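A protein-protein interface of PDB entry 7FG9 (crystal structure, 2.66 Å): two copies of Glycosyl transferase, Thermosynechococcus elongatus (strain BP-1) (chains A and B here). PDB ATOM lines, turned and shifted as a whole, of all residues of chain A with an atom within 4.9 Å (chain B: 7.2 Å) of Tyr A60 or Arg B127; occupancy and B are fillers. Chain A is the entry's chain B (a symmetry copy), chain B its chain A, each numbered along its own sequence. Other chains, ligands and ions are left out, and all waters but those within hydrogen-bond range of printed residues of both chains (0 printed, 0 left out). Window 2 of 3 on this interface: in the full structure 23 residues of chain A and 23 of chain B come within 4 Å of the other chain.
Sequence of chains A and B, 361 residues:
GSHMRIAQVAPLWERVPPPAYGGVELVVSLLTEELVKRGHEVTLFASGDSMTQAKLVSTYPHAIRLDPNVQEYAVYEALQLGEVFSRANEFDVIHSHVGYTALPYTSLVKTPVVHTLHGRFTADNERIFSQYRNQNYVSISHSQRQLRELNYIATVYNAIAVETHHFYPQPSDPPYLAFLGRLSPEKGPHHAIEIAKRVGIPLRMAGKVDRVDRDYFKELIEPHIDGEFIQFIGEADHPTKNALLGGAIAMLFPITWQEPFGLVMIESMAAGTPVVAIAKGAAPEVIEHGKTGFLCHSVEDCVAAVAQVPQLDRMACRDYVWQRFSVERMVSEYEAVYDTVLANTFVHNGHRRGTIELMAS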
ATOM      1  N   SER A  47       0.840 -22.961  -9.880  1.00  0.00           N
ATOM      2  CA  SER A  47       1.141 -22.874  -8.455  1.00  0.00           C
ATOM      3  C   SER A  47       1.963 -24.080  -7.991  1.00  0.00           C
ATOM      4  O   SER A  47       1.893 -25.170  -8.572  1.00  0.00           O
ATOM      5  CB  SER A  47      -0.146 -22.770  -7.631  1.00  0.00           C
ATOM      6  OG  SER A  47      -0.977 -23.920  -7.771  1.00  0.00           O
ATOM      7  N   GLY A  48       2.743 -23.868  -6.917  1.00  0.00           N
ATOM      8  CA  GLY A  48       3.659 -24.897  -6.432  1.00  0.00           C
ATOM      9  C   GLY A  48       2.980 -26.149  -5.904  1.00  0.00           C
ATOM     10  O   GLY A  48       3.574 -27.235  -5.900  1.00  0.00           O
ATOM     11  N   SER A  58       7.199 -22.873 -10.566  1.00  0.00           N
ATOM     12  CA  SER A  58       6.213 -22.178  -9.761  1.00  0.00           C
ATOM     13  C   SER A  58       6.836 -20.933  -9.146  1.00  0.00           C
ATOM     14  O   SER A  58       8.010 -20.936  -8.757  1.00  0.00           O
ATOM     15  CB  SER A  58       5.639 -23.102  -8.682  1.00  0.00           C
ATOM     16  OG  SER A  58       6.579 -23.347  -7.645  1.00  0.00           O
ATOM     17  N   THR A  59       6.049 -19.862  -9.079  1.00  0.00           N
ATOM     18  CA  THR A  59       6.527 -18.619  -8.494  1.00  0.00           C
ATOM     19  C   THR A  59       5.940 -18.378  -7.117  1.00  0.00           C
ATOM     20  O   THR A  59       6.311 -17.402  -6.459  1.00  0.00           O
ATOM     21  CB  THR A  59       6.212 -17.431  -9.419  1.00  0.00           C
ATOM     22  OG1 THR A  59       4.783 -17.239  -9.512  1.00  0.00           O
ATOM     23  CG2 THR A  59       6.825 -17.681 -10.828  1.00  0.00           C
ATOM     24  N   TYR A  60       5.030 -19.242  -6.669  1.00  0.00           N
ATOM     25  CA  TYR A  60       4.526 -19.155  -5.314  1.00  0.00           C
ATOM     26  C   TYR A  60       3.978 -20.524  -4.939  1.00  0.00           C
ATOM     27  O   TYR A  60       3.434 -21.216  -5.811  1.00  0.00           O
ATOM     28  CB  TYR A  60       3.455 -18.064  -5.188  1.00  0.00           C
ATOM     29  CG  TYR A  60       2.996 -17.862  -3.773  1.00  0.00           C
ATOM     30  CD1 TYR A  60       1.849 -18.492  -3.306  1.00  0.00           C
ATOM     31  CD2 TYR A  60       3.733 -17.087  -2.882  1.00  0.00           C
ATOM     32  CE1 TYR A  60       1.428 -18.342  -1.999  1.00  0.00           C
ATOM     33  CE2 TYR A  60       3.318 -16.928  -1.569  1.00  0.00           C
ATOM     34  CZ  TYR A  60       2.163 -17.560  -1.135  1.00  0.00           C
ATOM     35  OH  TYR A  60       1.727 -17.429   0.165  1.00  0.00           O
ATOM     36  N   PRO A  61       4.126 -20.960  -3.684  1.00  0.00           N
ATOM     37  CA  PRO A  61       3.814 -22.356  -3.335  1.00  0.00           C
ATOM     38  C   PRO A  61       2.341 -22.717  -3.233  1.00  0.00           C
ATOM     39  O   PRO A  61       2.053 -23.893  -2.985  1.00  0.00           O
ATOM     40  CB  PRO A  61       4.465 -22.532  -1.953  1.00  0.00           C
ATOM     41  CG  PRO A  61       5.187 -21.287  -1.646  1.00  0.00           C
ATOM     42  CD  PRO A  61       4.843 -20.242  -2.614  1.00  0.00           C
ATOM     43  N   HIS A  62       1.399 -21.781  -3.367  1.00  0.00           N
ATOM     44  CA  HIS A  62      -0.013 -22.089  -3.159  1.00  0.00           C
ATOM     45  C   HIS A  62      -0.855 -21.334  -4.167  1.00  0.00           C
ATOM     46  O   HIS A  62      -0.510 -20.217  -4.570  1.00  0.00           O
ATOM     47  CB  HIS A  62      -0.516 -21.709  -1.753  1.00  0.00           C
ATOM     48  CG  HIS A  62       0.252 -22.345  -0.636  1.00  0.00           C
ATOM     49  ND1 HIS A  62       0.096 -23.670  -0.286  1.00  0.00           N
ATOM     50  CD2 HIS A  62       1.177 -21.837   0.212  1.00  0.00           C
ATOM     51  CE1 HIS A  62       0.898 -23.950   0.726  1.00  0.00           C
ATOM     52  NE2 HIS A  62       1.561 -22.854   1.050  1.00  0.00           N
ATOM     53  N   ILE A  64      -3.674 -18.922  -5.455  1.00  0.00           N
ATOM     54  CA  ILE A  64      -3.804 -17.590  -4.865  1.00  0.00           C
ATOM     55  C   ILE A  64      -5.163 -17.387  -4.193  1.00  0.00           C
ATOM     56  O   ILE A  64      -5.253 -16.698  -3.170  1.00  0.00           O
ATOM     57  CB  ILE A  64      -3.540 -16.510  -5.931  1.00  0.00           C
ATOM     58  CG1 ILE A  64      -2.093 -16.547  -6.423  1.00  0.00           C
ATOM     59  CG2 ILE A  64      -3.904 -15.143  -5.399  1.00  0.00           C
ATOM     60  CD1 ILE A  64      -1.095 -16.549  -5.335  1.00  0.00           C
ATOM     61  N   ASP A  67      -5.741 -19.046  -0.812  1.00  0.00           N
ATOM     62  CA  ASP A  67      -4.789 -18.558   0.189  1.00  0.00           C
ATOM     63  C   ASP A  67      -5.244 -17.189   0.713  1.00  0.00           C
ATOM     64  O   ASP A  67      -5.598 -16.303  -0.089  1.00  0.00           O
ATOM     65  CB  ASP A  67      -3.387 -18.466  -0.398  1.00  0.00           C
ATOM     66  CG  ASP A  67      -2.314 -18.328   0.660  1.00  0.00           C
ATOM     67  OD1 ASP A  67      -2.470 -17.480   1.561  1.00  0.00           O
ATOM     68  OD2 ASP A  67      -1.303 -19.052   0.591  1.00  0.00           O
ATOM     69  N   ASN A  69      -3.235 -15.252   2.762  1.00  0.00           N
ATOM     70  CA  ASN A  69      -2.041 -14.430   2.915  1.00  0.00           C
ATOM     71  C   ASN A  69      -1.611 -13.760   1.619  1.00  0.00           C
ATOM     72  O   ASN A  69      -0.562 -13.106   1.598  1.00  0.00           O
ATOM     73  CB  ASN A  69      -0.882 -15.275   3.451  1.00  0.00           C
ATOM     74  CG  ASN A  69      -1.268 -16.089   4.673  1.00  0.00           C
ATOM     75  OD1 ASN A  69      -1.964 -15.603   5.573  1.00  0.00           O
ATOM     76  ND2 ASN A  69      -0.818 -17.344   4.707  1.00  0.00           N
ATOM     77  N   VAL A  70      -2.377 -13.919   0.540  1.00  0.00           N
ATOM     78  CA  VAL A  70      -2.039 -13.349  -0.761  1.00  0.00           C
ATOM     79  C   VAL A  70      -3.305 -12.741  -1.338  1.00  0.00           C
ATOM     80  O   VAL A  70      -4.405 -13.255  -1.113  1.00  0.00           O
ATOM     81  CB  VAL A  70      -1.433 -14.406  -1.709  1.00  0.00           C
ATOM     82  CG1 VAL A  70      -0.200 -15.050  -1.079  1.00  0.00           C
ATOM     83  CG2 VAL A  70      -2.449 -15.476  -2.058  1.00  0.00           C
ATOM     84  N   VAL A  75       0.795  -9.344  -9.146  1.00  0.00           N
ATOM     85  CA  VAL A  75       2.197  -9.594  -8.807  1.00  0.00           C
ATOM     86  C   VAL A  75       2.638 -10.947  -9.338  1.00  0.00           C
ATOM     87  O   VAL A  75       3.738 -11.093  -9.890  1.00  0.00           O
ATOM     88  CB  VAL A  75       2.407  -9.514  -7.283  1.00  0.00           C
ATOM     89  CG1 VAL A  75       3.675 -10.272  -6.891  1.00  0.00           C
ATOM     90  CG2 VAL A  75       2.467  -8.083  -6.831  1.00  0.00           C
ATOM     91  N   TYR A  76       1.782 -11.955  -9.181  1.00  0.00           N
ATOM     92  CA  TYR A  76       2.148 -13.321  -9.531  1.00  0.00           C
ATOM     93  C   TYR A  76       2.009 -13.585 -11.022  1.00  0.00           C
ATOM     94  O   TYR A  76       2.830 -14.315 -11.598  1.00  0.00           O
ATOM     95  CB  TYR A  76       1.317 -14.279  -8.688  1.00  0.00           C
ATOM     96  CG  TYR A  76       1.524 -13.972  -7.222  1.00  0.00           C
ATOM     97  CD1 TYR A  76       0.593 -13.243  -6.494  1.00  0.00           C
ATOM     98  CD2 TYR A  76       2.699 -14.361  -6.584  1.00  0.00           C
ATOM     99  CE1 TYR A  76       0.811 -12.947  -5.155  1.00  0.00           C
ATOM    100  CE2 TYR A  76       2.933 -14.067  -5.251  1.00  0.00           C
ATOM    101  CZ  TYR A  76       1.993 -13.362  -4.538  1.00  0.00           C
ATOM    102  OH  TYR A  76       2.244 -13.082  -3.206  1.00  0.00           O
ATOM    103  N   LEU A  79       5.319 -12.267 -12.342  1.00  0.00           N
ATOM    104  CA  LEU A  79       6.396 -13.217 -12.068  1.00  0.00           C
ATOM    105  C   LEU A  79       6.379 -14.367 -13.066  1.00  0.00           C
ATOM    106  O   LEU A  79       7.407 -14.710 -13.660  1.00  0.00           O
ATOM    107  CB  LEU A  79       6.266 -13.767 -10.647  1.00  0.00           C
ATOM    108  CG  LEU A  79       6.758 -12.887  -9.514  1.00  0.00           C
ATOM    109  CD1 LEU A  79       6.241 -13.388  -8.187  1.00  0.00           C
ATOM    110  CD2 LEU A  79       8.281 -12.864  -9.539  1.00  0.00           C
ATOM    111  N   THR B 122       4.606  -4.289  -0.080  1.00  0.00           N
ATOM    112  CA  THR B 122       3.678  -5.199   0.583  1.00  0.00           C
ATOM    113  C   THR B 122       4.294  -6.597   0.626  1.00  0.00           C
ATOM    114  O   THR B 122       5.265  -6.892  -0.076  1.00  0.00           O
ATOM    115  CB  THR B 122       2.313  -5.250  -0.124  1.00  0.00           C
ATOM    116  OG1 THR B 122       2.451  -5.955  -1.374  1.00  0.00           O
ATOM    117  CG2 THR B 122       1.720  -3.849  -0.347  1.00  0.00           C
ATOM    118  N   ALA B 123       3.721  -7.468   1.467  1.00  0.00           N
ATOM    119  CA  ALA B 123       4.171  -8.857   1.472  1.00  0.00           C
ATOM    120  C   ALA B 123       4.066  -9.466   0.085  1.00  0.00           C
ATOM    121  O   ALA B 123       4.892 -10.300  -0.285  1.00  0.00           O
ATOM    122  CB  ALA B 123       3.373  -9.691   2.474  1.00  0.00           C
ATOM    123  N   ASP B 124       3.080  -9.041  -0.706  1.00  0.00           N
ATOM    124  CA  ASP B 124       2.937  -9.577  -2.050  1.00  0.00           C
ATOM    125  C   ASP B 124       3.971  -8.985  -3.013  1.00  0.00           C
ATOM    126  O   ASP B 124       4.699  -9.736  -3.672  1.00  0.00           O
ATOM    127  CB  ASP B 124       1.511  -9.344  -2.558  1.00  0.00           C
ATOM    128  CG  ASP B 124       0.505 -10.337  -1.973  1.00  0.00           C
ATOM    129  OD1 ASP B 124       0.891 -11.494  -1.678  1.00  0.00           O
ATOM    130  OD2 ASP B 124      -0.684  -9.960  -1.830  1.00  0.00           O
ATOM    131  N   ASN B 125       4.074  -7.646  -3.116  1.00  0.00           N
ATOM    132  CA  ASN B 125       4.954  -7.119  -4.160  1.00  0.00           C
ATOM    133  C   ASN B 125       6.438  -7.244  -3.829  1.00  0.00           C
ATOM    134  O   ASN B 125       7.265  -7.117  -4.741  1.00  0.00           O
ATOM    135  CB  ASN B 125       4.622  -5.659  -4.537  1.00  0.00           C
ATOM    136  CG  ASN B 125       4.865  -4.625  -3.410  1.00  0.00           C
ATOM    137  OD1 ASN B 125       5.820  -4.690  -2.635  1.00  0.00           O
ATOM    138  ND2 ASN B 125       3.982  -3.639  -3.358  1.00  0.00           N
ATOM    139  N   GLU B 126       6.811  -7.515  -2.573  1.00  0.00           N
ATOM    140  CA  GLU B 126       8.221  -7.807  -2.324  1.00  0.00           C
ATOM    141  C   GLU B 126       8.678  -9.045  -3.085  1.00  0.00           C
ATOM    142  O   GLU B 126       9.842  -9.121  -3.494  1.00  0.00           O
ATOM    143  CB  GLU B 126       8.486  -7.960  -0.829  1.00  0.00           C
ATOM    144  CG  GLU B 126       8.443  -6.614  -0.100  1.00  0.00           C
ATOM    145  CD  GLU B 126       8.493  -6.725   1.413  1.00  0.00           C
ATOM    146  OE1 GLU B 126       8.401  -7.856   1.950  1.00  0.00           O
ATOM    147  OE2 GLU B 126       8.611  -5.664   2.070  1.00  0.00           O
ATOM    148  N   ARG B 127       7.772 -10.000  -3.330  1.00  0.00           N
ATOM    149  CA  ARG B 127       8.160 -11.204  -4.056  1.00  0.00           C
ATOM    150  C   ARG B 127       8.594 -10.905  -5.494  1.00  0.00           C
ATOM    151  O   ARG B 127       9.516 -11.554  -6.013  1.00  0.00           O
ATOM    152  CB  ARG B 127       7.027 -12.230  -4.008  1.00  0.00           C
ATOM    153  CG  ARG B 127       6.887 -12.813  -2.601  1.00  0.00           C
ATOM    154  CD  ARG B 127       5.938 -14.009  -2.469  1.00  0.00           C
ATOM    155  NE  ARG B 127       5.773 -14.385  -1.056  1.00  0.00           N
ATOM    156  CZ  ARG B 127       4.781 -13.960  -0.268  1.00  0.00           C
ATOM    157  NH1 ARG B 127       3.839 -13.147  -0.743  1.00  0.00           N
ATOM    158  NH2 ARG B 127       4.724 -14.343   1.000  1.00  0.00           N
ATOM    159  N   ILE B 128       7.996  -9.917  -6.150  1.00  0.00           N
ATOM    160  CA  ILE B 128       8.451  -9.669  -7.514  1.00  0.00           C
ATOM    161  C   ILE B 128       9.633  -8.707  -7.548  1.00  0.00           C
ATOM    162  O   ILE B 128      10.529  -8.856  -8.386  1.00  0.00           O
ATOM    163  CB  ILE B 128       7.298  -9.176  -8.403  1.00  0.00           C
ATOM    164  CG1 ILE B 128       7.809  -9.039  -9.832  1.00  0.00           C
ATOM    165  CG2 ILE B 128       6.745  -7.865  -7.880  1.00  0.00           C
ATOM    166  CD1 ILE B 128       6.751  -9.012 -10.859  1.00  0.00           C
ATOM    167  N   PHE B 129       9.670  -7.710  -6.650  1.00  0.00           N
ATOM    168  CA  PHE B 129      10.807  -6.790  -6.624  1.00  0.00           C
ATOM    169  C   PHE B 129      12.088  -7.523  -6.254  1.00  0.00           C
ATOM    170  O   PHE B 129      13.141  -7.305  -6.867  1.00  0.00           O
ATOM    171  CB  PHE B 129      10.541  -5.640  -5.651  1.00  0.00           C
ATOM    172  CG  PHE B 129       9.625  -4.585  -6.201  1.00  0.00           C
ATOM    173  CD1 PHE B 129       9.983  -3.851  -7.306  1.00  0.00           C
ATOM    174  CD2 PHE B 129       8.393  -4.345  -5.621  1.00  0.00           C
ATOM    175  CE1 PHE B 129       9.135  -2.884  -7.811  1.00  0.00           C
ATOM    176  CE2 PHE B 129       7.543  -3.382  -6.131  1.00  0.00           C
ATOM    177  CZ  PHE B 129       7.914  -2.652  -7.222  1.00  0.00           C
ATOM    178  N   SER B 130      12.003  -8.417  -5.268  1.00  0.00           N
ATOM    179  CA  SER B 130      13.129  -9.271  -4.911  1.00  0.00           C
ATOM    180  C   SER B 130      13.653 -10.064  -6.113  1.00  0.00           C
ATOM    181  O   SER B 130      14.869 -10.184  -6.296  1.00  0.00           O
ATOM    182  CB  SER B 130      12.697 -10.200  -3.777  1.00  0.00           C
ATOM    183  OG  SER B 130      13.807 -10.817  -3.174  1.00  0.00           O
ATOM    184  N   GLN B 131      12.758 -10.607  -6.952  1.00  0.00           N
ATOM    185  CA  GLN B 131      13.193 -11.351  -8.136  1.00  0.00           C
ATOM    186  C   GLN B 131      13.930 -10.485  -9.134  1.00  0.00           C
ATOM    187  O   GLN B 131      14.621 -11.019 -10.009  1.00  0.00           O
ATOM    188  CB  GLN B 131      12.011 -11.975  -8.866  1.00  0.00           C
ATOM    189  CG  GLN B 131      11.635 -13.341  -8.401  1.00  0.00           C
ATOM    190  CD  GLN B 131      12.601 -14.381  -8.880  1.00  0.00           C
ATOM    191  OE1 GLN B 131      13.099 -15.195  -8.097  1.00  0.00           O
ATOM    192  NE2 GLN B 131      12.903 -14.346 -10.177  1.00  0.00           N
ATOM    193  N   TYR B 132      13.751  -9.171  -9.057  1.00  0.00           N
ATOM    194  CA  TYR B 132      14.328  -8.226 -10.002  1.00  0.00           C
ATOM    195  C   TYR B 132      15.116  -7.159  -9.255  1.00  0.00           C
ATOM    196  O   TYR B 132      15.143  -5.987  -9.640  1.00  0.00           O
ATOM    197  CB  TYR B 132      13.243  -7.616 -10.884  1.00  0.00           C
ATOM    198  CG  TYR B 132      12.568  -8.617 -11.800  1.00  0.00           C
ATOM    199  CD1 TYR B 132      13.156  -8.986 -13.013  1.00  0.00           C
ATOM    200  CD2 TYR B 132      11.337  -9.189 -11.469  1.00  0.00           C
ATOM    201  CE1 TYR B 132      12.545  -9.895 -13.870  1.00  0.00           C
ATOM    202  CE2 TYR B 132      10.706 -10.111 -12.326  1.00  0.00           C
ATOM    203  CZ  TYR B 132      11.320 -10.456 -13.531  1.00  0.00           C
ATOM    204  OH  TYR B 132      10.724 -11.359 -14.404  1.00  0.00           O
ATOM    205  N   LEU B 147      12.697  -2.802   1.449  1.00  0.00           N
ATOM    206  CA  LEU B 147      13.289  -4.073   1.033  1.00  0.00           C
ATOM    207  C   LEU B 147      14.749  -4.218   1.449  1.00  0.00           C
ATOM    208  O   LEU B 147      15.118  -5.224   2.085  1.00  0.00           O
ATOM    209  CB  LEU B 147      13.158  -4.293  -0.470  1.00  0.00           C
ATOM    210  CG  LEU B 147      11.959  -5.147  -0.840  1.00  0.00           C
ATOM    211  CD1 LEU B 147      11.885  -5.284  -2.333  1.00  0.00           C
ATOM    212  CD2 LEU B 147      12.186  -6.504  -0.230  1.00  0.00           C
ATOM    213  N   GLU B 149      17.555  -5.032   0.021  1.00  0.00           N
ATOM    214  CA  GLU B 149      18.248  -5.805  -1.004  1.00  0.00           C
ATOM    215  C   GLU B 149      18.128  -5.240  -2.438  1.00  0.00           C
ATOM    216  O   GLU B 149      18.510  -5.983  -3.346  1.00  0.00           O
ATOM    217  CB  GLU B 149      17.694  -7.225  -0.999  1.00  0.00           C
ATOM    218  CG  GLU B 149      16.170  -7.249  -0.931  1.00  0.00           C
ATOM    219  CD  GLU B 149      15.576  -8.591  -1.327  1.00  0.00           C
ATOM    220  OE1 GLU B 149      16.289  -9.406  -1.967  1.00  0.00           O
ATOM    221  OE2 GLU B 149      14.391  -8.829  -0.994  1.00  0.00           O
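Ser A58 touches none of the printed residues of chain B.
Of chain B, only Arg B127 (3.6 Å) comes within 4 Å of Tyr A60.
Of the printed residues of chain B, Asn A69 touches Asp B124.
Of the printed residues of chain B, Tyr A76 touches Asp B124 (2.6 Å) and Arg B127 (2.9 Å).
Printed residues of chain A within 4 Å of Asp B124: Asn A69, Val A70, Val A75 and Tyr A76.
Of chain A, only Tyr A60, Tyr A76 and Leu A79 come within 4 Å of Arg B127.
The nearest printed residue of chain A that does not touch Asp B124 is Tyr A60 (6.0 Å).
OD1 of Asp A67 is in hydrogen-bond range of N of Asn A69, 2.6 Å away.
O of Tyr A60 sits at hydrogen-bond distance from N of Gly A48, 3.0 Å away.
The side-chain hydroxyl (OH) of Tyr A60 sits at hydrogen-bond distance from the side-chain carboxylate (OD2) of Asp A67 (3.5 Å).
The backbone carbonyl oxygen (O) of Ala B123 sits at hydrogen-bond distance from the guanidinium group (NH1) of Arg B127 (3.1 Å).
The guanidinium group (NH1) of Arg B127 lies within salt-bridge range of the side-chain carboxylate (OD1) of Asp B124 (3.5 Å).
The side-chain amide oxygen (OD1) of Asn B125 is in hydrogen-bond range of the backbone NH (N) of Thr B122 (2.9 Å).
Hydrophobic or aromatic side chains of chain B that line the printed part of chain A: Ile B128.
Hydrophobic or aromatic side chains of chain A that line the printed part of chain B: Tyr A60, Val A70, Val A75, Tyr A76 and Leu A79.
Among the printed residues, 11 pairs touch across the chains.
Among the printed residues, no Asp or Glu carboxylate lies within 4 Å of a Lys or Arg side-chain nitrogen of the other chain.
The guanidinium group (NH1) of Arg B127 sits at hydrogen-bond distance from the side-chain hydroxyl (OH) of Tyr A76.
The side-chain carboxylate (OD1) of Asp B124 is in hydrogen-bond range of the side-chain hydroxyl (OH) of Tyr A76 (2.6 Å).
Among the printed residues, merely in contact across the chains: Tyr A60 with Arg B127 (3.6 Å), Asn A69 with Asp B124 (3.9 Å), Val A70 with Asp B124 (3.6 Å), Val A75 with Asp B124 (3.4 Å), Val A75 with Asn B125 (3.8 Å), Val A75 with Ile B128 (3.8 Å), Leu A79 with Arg B127 (3.96 Å), Leu A79 with Ile B128 (3.8 Å) and Leu A79 with Gln B131 (3.6 Å).
No position is printed for both chains.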
